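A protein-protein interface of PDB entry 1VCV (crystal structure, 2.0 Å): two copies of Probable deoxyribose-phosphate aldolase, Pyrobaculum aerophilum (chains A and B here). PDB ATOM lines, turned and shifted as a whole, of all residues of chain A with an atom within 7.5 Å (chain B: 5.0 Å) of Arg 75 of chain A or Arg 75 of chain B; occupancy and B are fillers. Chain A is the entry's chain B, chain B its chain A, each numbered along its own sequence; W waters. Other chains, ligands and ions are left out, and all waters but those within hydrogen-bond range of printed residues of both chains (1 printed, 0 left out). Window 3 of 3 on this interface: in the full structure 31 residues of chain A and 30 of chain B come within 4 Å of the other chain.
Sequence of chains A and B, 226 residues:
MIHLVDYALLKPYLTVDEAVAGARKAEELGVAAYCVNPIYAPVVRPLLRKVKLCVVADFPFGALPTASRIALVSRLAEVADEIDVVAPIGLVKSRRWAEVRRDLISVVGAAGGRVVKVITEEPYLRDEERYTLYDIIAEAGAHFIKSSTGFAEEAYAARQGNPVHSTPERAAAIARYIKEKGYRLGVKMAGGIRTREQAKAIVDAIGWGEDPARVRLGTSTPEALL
The guanidinium group (NH1) of Arg 75 of chain B sits close to the backbone carbonyl oxygen (O) of Ala 71 of chain B (3.4 Å).
Ser 68 of chain A touches Leu 72 of chain B, and with the chains exchanged Leu 72 of chain A touches Ser 68 of chain B.
Ser 68 of chain A touches Arg 75 of chain B, and with the chains exchanged Arg 75 of chain A touches Ser 68 of chain B.
Ala 71 of chain A touches Arg 75 of chain B, and with the chains exchanged Arg 75 of chain A touches Ala 71 of chain B.
Arg 75 of chain B touches its own counterpart, Arg 75 of chain A.
11 positions are printed for both chains.
The guanidinium group (NH1) of Arg 75 of chain B lies within hydrogen-bond range of the side-chain hydroxyl (OG) of Ser 68 of chain A (3.4 Å).
The guanidinium group (NH2) of Arg 75 of chain A sits close to the guanidinium group (NH2) of Arg 75 of chain B (2.7 Å).
Water W1 bridges the guanidinium group of Arg 75 of chain A (2.6 Å) and the guanidinium group of Arg 75 of chain B (2.7 Å).
Ile 70 of chain A touches none of the printed residues of chain B.
Arg 75 of chain A touches just these residues of chain B: Ser 68 (3.7 Å), Ala 71 (3.2 Å) and Arg 75 (2.7 Å).
Of the printed residues of chain A, Ser 68 of chain B touches Leu 72 (3.4 Å) and Arg 75 (3.7 Å).
Of the printed residues of chain A, Leu 72 of chain B touches Leu 64 and Ser 68.
Val 73 of chain B touches none of the printed residues of chain A.
Of the printed residues of chain A, Arg 75 of chain B touches Ser 68 (3.4 Å), Ala 71 (2.9 Å) and Arg 75 (2.7 Å).
The nearest residue of chain B that does not touch Arg 75 of chain A is Ala 67 of chain B (4.9 Å).
The nearest residue of chain A that does not touch Arg 75 of chain B is Ala 67 of chain A (4.7 Å).
The nearest printed residue of chain A that does not touch Ala 71 of chain B is Ser 68 of chain A (6.0 Å).
Hydrophobic or aromatic side chains of chain A that line the printed part of chain B: Leu 64, Ala 71 and Leu 72.
Of the 11 printed residues of chain B, 4 touch a printed residue of chain A.
Hydrophobic or aromatic side chains of chain B within 4 Å of the printed part of chain A: Ala 71 and Leu 72.
Among the printed residues, 8 pairs touch across the chains.
Among the printed residues, no Asp or Glu carboxylate lies within 4 Å of a Lys or Arg side-chain nitrogen of the other chain.
Leu 64 of chain A touches Leu 72 of chain B.
OG of Ser 68 of chain A touches CD1 of Leu 72 of chain B (3.7 Å).
Ala 71 of chain A touches Arg 75 of chain B.
Ser 68 of chain B touches Leu 72 of chain A.
Arg 75 of chain A touches Ser 68 of chain B (NH1 to OG, 3.7 Å).
Arg 75 of chain A touches Ala 71 of chain B (NH2 to CB, 3.2 Å).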
ATOM      1  N   LEU A  64       3.413 -11.089 -21.132  1.00  0.00           N
ATOM      2  CA  LEU A  64       1.969 -11.277 -21.240  1.00  0.00           C
ATOM      3  C   LEU A  64       1.764 -12.535 -22.082  1.00  0.00           C
ATOM      4  O   LEU A  64       2.665 -12.956 -22.811  1.00  0.00           O
ATOM      5  CB  LEU A  64       1.299 -10.093 -21.948  1.00  0.00           C
ATOM      6  CG  LEU A  64       0.993  -8.802 -21.182  1.00  0.00           C
ATOM      7  CD1 LEU A  64       0.502  -7.738 -22.153  1.00  0.00           C
ATOM      8  CD2 LEU A  64      -0.052  -9.074 -20.114  1.00  0.00           C
ATOM      9  N   PRO A  65       0.591 -13.174 -21.970  1.00  0.00           N
ATOM     10  CA  PRO A  65       0.390 -14.370 -22.791  1.00  0.00           C
ATOM     11  C   PRO A  65       0.322 -13.915 -24.255  1.00  0.00           C
ATOM     12  O   PRO A  65       0.005 -12.760 -24.531  1.00  0.00           O
ATOM     13  CB  PRO A  65      -0.935 -14.929 -22.266  1.00  0.00           C
ATOM     14  CG  PRO A  65      -1.649 -13.714 -21.777  1.00  0.00           C
ATOM     15  CD  PRO A  65      -0.563 -12.929 -21.089  1.00  0.00           C
ATOM     16  N   ALA A  67      -1.831 -14.377 -26.732  1.00  0.00           N
ATOM     17  CA  ALA A  67      -3.110 -13.808 -27.168  1.00  0.00           C
ATOM     18  C   ALA A  67      -3.237 -12.323 -26.814  1.00  0.00           C
ATOM     19  O   ALA A  67      -3.656 -11.511 -27.644  1.00  0.00           O
ATOM     20  CB  ALA A  67      -4.273 -14.596 -26.562  1.00  0.00           C
ATOM     21  N   SER A  68      -2.867 -11.961 -25.588  1.00  0.00           N
ATOM     22  CA  SER A  68      -2.957 -10.562 -25.170  1.00  0.00           C
ATOM     23  C   SER A  68      -1.981  -9.704 -25.952  1.00  0.00           C
ATOM     24  O   SER A  68      -2.291  -8.566 -26.302  1.00  0.00           O
ATOM     25  CB  SER A  68      -2.668 -10.418 -23.674  1.00  0.00           C
ATOM     26  OG  SER A  68      -3.652 -11.077 -22.904  1.00  0.00           O
ATOM     27  N   ARG A  69      -0.796 -10.251 -26.218  1.00  0.00           N
ATOM     28  CA  ARG A  69       0.225  -9.524 -26.962  1.00  0.00           C
ATOM     29  C   ARG A  69      -0.268  -9.246 -28.378  1.00  0.00           C
ATOM     30  O   ARG A  69      -0.081  -8.146 -28.904  1.00  0.00           O
ATOM     31  CB  ARG A  69       1.541 -10.319 -26.981  1.00  0.00           C
ATOM     32  CG  ARG A  69       2.321 -10.232 -25.663  1.00  0.00           C
ATOM     33  CD  ARG A  69       3.243 -11.425 -25.458  1.00  0.00           C
ATOM     34  NE  ARG A  69       4.302 -11.513 -26.465  1.00  0.00           N
ATOM     35  CZ  ARG A  69       5.315 -10.659 -26.567  1.00  0.00           C
ATOM     36  NH1 ARG A  69       5.418  -9.636 -25.722  1.00  0.00           N
ATOM     37  NH2 ARG A  69       6.235 -10.832 -27.511  1.00  0.00           N
ATOM     38  N   ILE A  70      -0.909 -10.237 -28.989  1.00  0.00           N
ATOM     39  CA  ILE A  70      -1.454 -10.076 -30.335  1.00  0.00           C
ATOM     40  C   ILE A  70      -2.515  -8.975 -30.342  1.00  0.00           C
ATOM     41  O   ILE A  70      -2.478  -8.059 -31.169  1.00  0.00           O
ATOM     42  CB  ILE A  70      -2.112 -11.382 -30.827  1.00  0.00           C
ATOM     43  CG1 ILE A  70      -1.031 -12.406 -31.187  1.00  0.00           C
ATOM     44  CG2 ILE A  70      -3.036 -11.095 -32.009  1.00  0.00           C
ATOM     45  CD1 ILE A  70      -1.584 -13.774 -31.549  1.00  0.00           C
ATOM     46  N   ALA A  71      -3.459  -9.079 -29.414  1.00  0.00           N
ATOM     47  CA  ALA A  71      -4.546  -8.115 -29.304  1.00  0.00           C
ATOM     48  C   ALA A  71      -3.999  -6.711 -29.094  1.00  0.00           C
ATOM     49  O   ALA A  71      -4.457  -5.749 -29.721  1.00  0.00           O
ATOM     50  CB  ALA A  71      -5.466  -8.501 -28.141  1.00  0.00           C
ATOM     51  N   LEU A  72      -3.007  -6.605 -28.213  1.00  0.00           N
ATOM     52  CA  LEU A  72      -2.388  -5.324 -27.906  1.00  0.00           C
ATOM     53  C   LEU A  72      -1.734  -4.694 -29.127  1.00  0.00           C
ATOM     54  O   LEU A  72      -1.960  -3.521 -29.428  1.00  0.00           O
ATOM     55  CB  LEU A  72      -1.339  -5.496 -26.805  1.00  0.00           C
ATOM     56  CG  LEU A  72      -0.757  -4.189 -26.264  1.00  0.00           C
ATOM     57  CD1 LEU A  72      -1.878  -3.362 -25.646  1.00  0.00           C
ATOM     58  CD2 LEU A  72       0.321  -4.489 -25.226  1.00  0.00           C
ATOM     59  N   VAL A  73      -0.913  -5.470 -29.822  1.00  0.00           N
ATOM     60  CA  VAL A  73      -0.231  -4.957 -30.995  1.00  0.00           C
ATOM     61  C   VAL A  73      -1.240  -4.575 -32.072  1.00  0.00           C
ATOM     62  O   VAL A  73      -1.069  -3.578 -32.775  1.00  0.00           O
ATOM     63  CB  VAL A  73       0.765  -5.989 -31.551  1.00  0.00           C
ATOM     64  CG1 VAL A  73       1.389  -5.470 -32.846  1.00  0.00           C
ATOM     65  CG2 VAL A  73       1.846  -6.258 -30.517  1.00  0.00           C
ATOM     66  N   SER A  74      -2.299  -5.366 -32.194  1.00  0.00           N
ATOM     67  CA  SER A  74      -3.325  -5.072 -33.182  1.00  0.00           C
ATOM     68  C   SER A  74      -3.939  -3.692 -32.908  1.00  0.00           C
ATOM     69  O   SER A  74      -4.077  -2.871 -33.822  1.00  0.00           O
ATOM     70  CB  SER A  74      -4.409  -6.153 -33.143  1.00  0.00           C
ATOM     71  OG  SER A  74      -5.295  -6.022 -34.237  1.00  0.00           O
ATOM     72  N   ARG A  75      -4.284  -3.430 -31.647  1.00  0.00           N
ATOM     73  CA  ARG A  75      -4.884  -2.150 -31.268  1.00  0.00           C
ATOM     74  C   ARG A  75      -3.913  -0.988 -31.444  1.00  0.00           C
ATOM     75  O   ARG A  75      -4.291   0.079 -31.932  1.00  0.00           O
ATOM     76  CB  ARG A  75      -5.362  -2.181 -29.811  1.00  0.00           C
ATOM     77  CG  ARG A  75      -6.327  -3.309 -29.486  1.00  0.00           C
ATOM     78  CD  ARG A  75      -7.080  -3.056 -28.180  1.00  0.00           C
ATOM     79  NE  ARG A  75      -7.760  -4.263 -27.713  1.00  0.00           N
ATOM     80  CZ  ARG A  75      -7.202  -5.177 -26.921  1.00  0.00           C
ATOM     81  NH1 ARG A  75      -5.952  -5.021 -26.494  1.00  0.00           N
ATOM     82  NH2 ARG A  75      -7.889  -6.256 -26.572  1.00  0.00           N
ATOM     83  N   LEU A  76      -2.663  -1.201 -31.037  1.00  0.00           N
ATOM     84  CA  LEU A  76      -1.631  -0.174 -31.139  1.00  0.00           C
ATOM     85  C   LEU A  76      -1.324   0.237 -32.572  1.00  0.00           C
ATOM     86  O   LEU A  76      -1.038   1.402 -32.837  1.00  0.00           O
ATOM     87  CB  LEU A  76      -0.348  -0.653 -30.449  1.00  0.00           C
ATOM     88  CG  LEU A  76      -0.222  -0.403 -28.939  1.00  0.00           C
ATOM     89  CD1 LEU A  76      -1.525  -0.704 -28.232  1.00  0.00           C
ATOM     90  CD2 LEU A  76       0.906  -1.260 -28.377  1.00  0.00           C
ATOM     91  N   ALA A  77      -1.387  -0.718 -33.494  1.00  0.00           N
ATOM     92  CA  ALA A  77      -1.106  -0.448 -34.900  1.00  0.00           C
ATOM     93  C   ALA A  77      -2.099   0.535 -35.510  1.00  0.00           C
ATOM     94  O   ALA A  77      -1.836   1.119 -36.557  1.00  0.00           O
ATOM     95  CB  ALA A  77      -1.118  -1.746 -35.695  1.00  0.00           C
ATOM     96  N   GLU A  78      -3.240   0.714 -34.857  1.00  0.00           N
ATOM     97  CA  GLU A  78      -4.260   1.623 -35.365  1.00  0.00           C
ATOM     98  C   GLU A  78      -3.909   3.097 -35.179  1.00  0.00           C
ATOM     99  O   GLU A  78      -4.444   3.955 -35.874  1.00  0.00           O
ATOM    100  CB  GLU A  78      -5.609   1.318 -34.702  1.00  0.00           C
ATOM    101  CG  GLU A  78      -6.237   0.000 -35.154  1.00  0.00           C
ATOM    102  CD  GLU A  78      -7.529  -0.317 -34.416  1.00  0.00           C
ATOM    103  OE1 GLU A  78      -8.396   0.577 -34.326  1.00  0.00           O
ATOM    104  OE2 GLU A  78      -7.679  -1.462 -33.930  1.00  0.00           O
ATOM    105  N   VAL A  79      -3.001   3.398 -34.258  1.00  0.00           N
ATOM    106  CA  VAL A  79      -2.631   4.789 -34.024  1.00  0.00           C
ATOM    107  C   VAL A  79      -1.134   5.069 -34.080  1.00  0.00           C
ATOM    108  O   VAL A  79      -0.725   6.215 -34.262  1.00  0.00           O
ATOM    109  CB  VAL A  79      -3.159   5.280 -32.661  1.00  0.00           C
ATOM    110  CG1 VAL A  79      -4.676   5.168 -32.625  1.00  0.00           C
ATOM    111  CG2 VAL A  79      -2.542   4.468 -31.538  1.00  0.00           C
ATOM    112  N   ALA A  80      -0.319   4.030 -33.933  1.00  0.00           N
ATOM    113  CA  ALA A  80       1.130   4.203 -33.960  1.00  0.00           C
ATOM    114  C   ALA A  80       1.747   3.868 -35.312  1.00  0.00           C
ATOM    115  O   ALA A  80       1.289   2.967 -36.008  1.00  0.00           O
ATOM    116  CB  ALA A  80       1.773   3.347 -32.877  1.00  0.00           C
ATOM    117  N   ILE A  83       6.021   0.192 -33.769  1.00  0.00           N
ATOM    118  CA  ILE A  83       5.788  -0.537 -32.531  1.00  0.00           C
ATOM    119  C   ILE A  83       6.998  -1.362 -32.093  1.00  0.00           C
ATOM    120  O   ILE A  83       7.433  -2.275 -32.801  1.00  0.00           O
ATOM    121  CB  ILE A  83       4.585  -1.487 -32.672  1.00  0.00           C
ATOM    122  CG1 ILE A  83       3.325  -0.682 -33.008  1.00  0.00           C
ATOM    123  CG2 ILE A  83       4.396  -2.282 -31.388  1.00  0.00           C
ATOM    124  CD1 ILE A  83       2.104  -1.541 -33.261  1.00  0.00           C
ATOM    125  N   ALA A 110       0.538  -9.173 -36.160  1.00  0.00           N
ATOM    126  CA  ALA A 110      -0.661  -8.500 -35.685  1.00  0.00           C
ATOM    127  C   ALA A 110      -0.525  -6.998 -35.880  1.00  0.00           C
ATOM    128  O   ALA A 110      -1.486  -6.253 -35.702  1.00  0.00           O
ATOM    129  CB  ALA A 110      -0.893  -8.819 -34.208  1.00  0.00           C
ATOM    130  N   ALA A 111       0.676  -6.563 -36.253  1.00  0.00           N
ATOM    131  CA  ALA A 111       0.962  -5.146 -36.468  1.00  0.00           C
ATOM    132  C   ALA A 111       0.368  -4.608 -37.764  1.00  0.00           C
ATOM    133  O   ALA A 111       0.371  -3.401 -38.001  1.00  0.00           O
ATOM    134  CB  ALA A 111       2.465  -4.920 -36.459  1.00  0.00           C
ATOM    135  N   ALA B  67      -8.513   1.035 -22.579  1.00  0.00           N
ATOM    136  CA  ALA B  67      -9.168   0.006 -23.384  1.00  0.00           C
ATOM    137  C   ALA B  67      -8.396  -1.316 -23.363  1.00  0.00           C
ATOM    138  O   ALA B  67      -8.992  -2.391 -23.270  1.00  0.00           O
ATOM    139  CB  ALA B  67      -9.336   0.491 -24.821  1.00  0.00           C
ATOM    140  N   SER B  68      -7.072  -1.241 -23.451  1.00  0.00           N
ATOM    141  CA  SER B  68      -6.258  -2.452 -23.424  1.00  0.00           C
ATOM    142  C   SER B  68      -6.243  -3.051 -22.023  1.00  0.00           C
ATOM    143  O   SER B  68      -6.188  -4.270 -21.856  1.00  0.00           O
ATOM    144  CB  SER B  68      -4.826  -2.145 -23.863  1.00  0.00           C
ATOM    145  OG  SER B  68      -4.806  -1.714 -25.206  1.00  0.00           O
ATOM    146  N   ALA B  71      -9.479  -4.963 -21.327  1.00  0.00           N
ATOM    147  CA  ALA B  71      -9.454  -6.183 -22.137  1.00  0.00           C
ATOM    148  C   ALA B  71      -8.526  -7.225 -21.520  1.00  0.00           C
ATOM    149  O   ALA B  71      -8.868  -8.403 -21.420  1.00  0.00           O
ATOM    150  CB  ALA B  71      -9.007  -5.859 -23.565  1.00  0.00           C
ATOM    151  N   LEU B  72      -7.347  -6.778 -21.104  1.00  0.00           N
ATOM    152  CA  LEU B  72      -6.365  -7.659 -20.492  1.00  0.00           C
ATOM    153  C   LEU B  72      -6.923  -8.288 -19.222  1.00  0.00           C
ATOM    154  O   LEU B  72      -6.878  -9.505 -19.047  1.00  0.00           O
ATOM    155  CB  LEU B  72      -5.102  -6.866 -20.153  1.00  0.00           C
ATOM    156  CG  LEU B  72      -4.116  -7.583 -19.238  1.00  0.00           C
ATOM    157  CD1 LEU B  72      -3.592  -8.834 -19.943  1.00  0.00           C
ATOM    158  CD2 LEU B  72      -2.976  -6.637 -18.882  1.00  0.00           C
ATOM    159  N   VAL B  73      -7.442  -7.445 -18.334  1.00  0.00           N
ATOM    160  CA  VAL B  73      -8.004  -7.908 -17.074  1.00  0.00           C
ATOM    161  C   VAL B  73      -9.129  -8.912 -17.323  1.00  0.00           C
ATOM    162  O   VAL B  73      -9.254  -9.912 -16.609  1.00  0.00           O
ATOM    163  CB  VAL B  73      -8.530  -6.714 -16.238  1.00  0.00           C
ATOM    164  CG1 VAL B  73      -9.255  -7.209 -14.995  1.00  0.00           C
ATOM    165  CG2 VAL B  73      -7.364  -5.819 -15.834  1.00  0.00           C
ATOM    166  N   SER B  74      -9.937  -8.645 -18.344  1.00  0.00           N
ATOM    167  CA  SER B  74     -11.041  -9.528 -18.690  1.00  0.00           C
ATOM    168  C   SER B  74     -10.519 -10.924 -19.040  1.00  0.00           C
ATOM    169  O   SER B  74     -11.027 -11.928 -18.535  1.00  0.00           O
ATOM    170  CB  SER B  74     -11.831  -8.946 -19.864  1.00  0.00           C
ATOM    171  OG  SER B  74     -13.039  -9.659 -20.058  1.00  0.00           O
ATOM    172  N   ARG B  75      -9.501 -10.996 -19.896  1.00  0.00           N
ATOM    173  CA  ARG B  75      -8.941 -12.296 -20.260  1.00  0.00           C
ATOM    174  C   ARG B  75      -8.376 -12.961 -19.020  1.00  0.00           C
ATOM    175  O   ARG B  75      -8.723 -14.092 -18.690  1.00  0.00           O
ATOM    176  CB  ARG B  75      -7.813 -12.160 -21.286  1.00  0.00           C
ATOM    177  CG  ARG B  75      -8.201 -11.471 -22.573  1.00  0.00           C
ATOM    178  CD  ARG B  75      -7.186 -11.761 -23.676  1.00  0.00           C
ATOM    179  NE  ARG B  75      -7.343 -10.819 -24.776  1.00  0.00           N
ATOM    180  CZ  ARG B  75      -6.950  -9.550 -24.718  1.00  0.00           C
ATOM    181  NH1 ARG B  75      -6.368  -9.082 -23.621  1.00  0.00           N
ATOM    182  NH2 ARG B  75      -7.164  -8.743 -25.746  1.00  0.00           N
ATOM    183  N   LEU B  76      -7.496 -12.238 -18.337  1.00  0.00           N
ATOM    184  CA  LEU B  76      -6.851 -12.739 -17.134  1.00  0.00           C
ATOM    185  C   LEU B  76      -7.827 -13.304 -16.109  1.00  0.00           C
ATOM    186  O   LEU B  76      -7.536 -14.306 -15.457  1.00  0.00           O
ATOM    187  CB  LEU B  76      -6.009 -11.624 -16.504  1.00  0.00           C
ATOM    188  CG  LEU B  76      -4.547 -11.529 -16.957  1.00  0.00           C
ATOM    189  CD1 LEU B  76      -4.438 -11.649 -18.461  1.00  0.00           C
ATOM    190  CD2 LEU B  76      -3.952 -10.218 -16.470  1.00  0.00           C
ATOM    191  N   ALA B  77      -8.984 -12.664 -15.973  1.00  0.00           N
ATOM    192  CA  ALA B  77      -9.992 -13.108 -15.018  1.00  0.00           C
ATOM    193  C   ALA B  77     -10.538 -14.494 -15.363  1.00  0.00           C
ATOM    194  O   ALA B  77     -11.185 -15.140 -14.539  1.00  0.00           O
ATOM    195  CB  ALA B  77     -11.130 -12.100 -14.962  1.00  0.00           C
ATOM    196  N   GLU B  78     -10.275 -14.955 -16.580  1.00  0.00           N
ATOM    197  CA  GLU B  78     -10.763 -16.267 -16.982  1.00  0.00           C
ATOM    198  C   GLU B  78     -10.022 -17.410 -16.299  1.00  0.00           C
ATOM    199  O   GLU B  78     -10.589 -18.481 -16.098  1.00  0.00           O
ATOM    200  CB  GLU B  78     -10.675 -16.427 -18.501  1.00  0.00           C
ATOM    201  CG  GLU B  78     -11.651 -15.548 -19.268  1.00  0.00           C
ATOM    202  CD  GLU B  78     -11.641 -15.833 -20.752  1.00  0.00           C
ATOM    203  OE1 GLU B  78     -11.771 -17.019 -21.120  1.00  0.00           O
ATOM    204  OE2 GLU B  78     -11.506 -14.880 -21.551  1.00  0.00           O
ATOM    205  N   VAL B  79      -8.767 -17.186 -15.919  1.00  0.00           N
ATOM    206  CA  VAL B  79      -7.999 -18.248 -15.274  1.00  0.00           C
ATOM    207  C   VAL B  79      -7.406 -17.925 -13.906  1.00  0.00           C
ATOM    208  O   VAL B  79      -7.146 -18.829 -13.114  1.00  0.00           O
ATOM    209  CB  VAL B  79      -6.858 -18.729 -16.187  1.00  0.00           C
ATOM    210  CG1 VAL B  79      -7.441 -19.445 -17.401  1.00  0.00           C
ATOM    211  CG2 VAL B  79      -6.015 -17.548 -16.629  1.00  0.00           C
HETATM  212  O   HOH W   1      -5.452  -6.922 -24.864  1.00  0.00           O
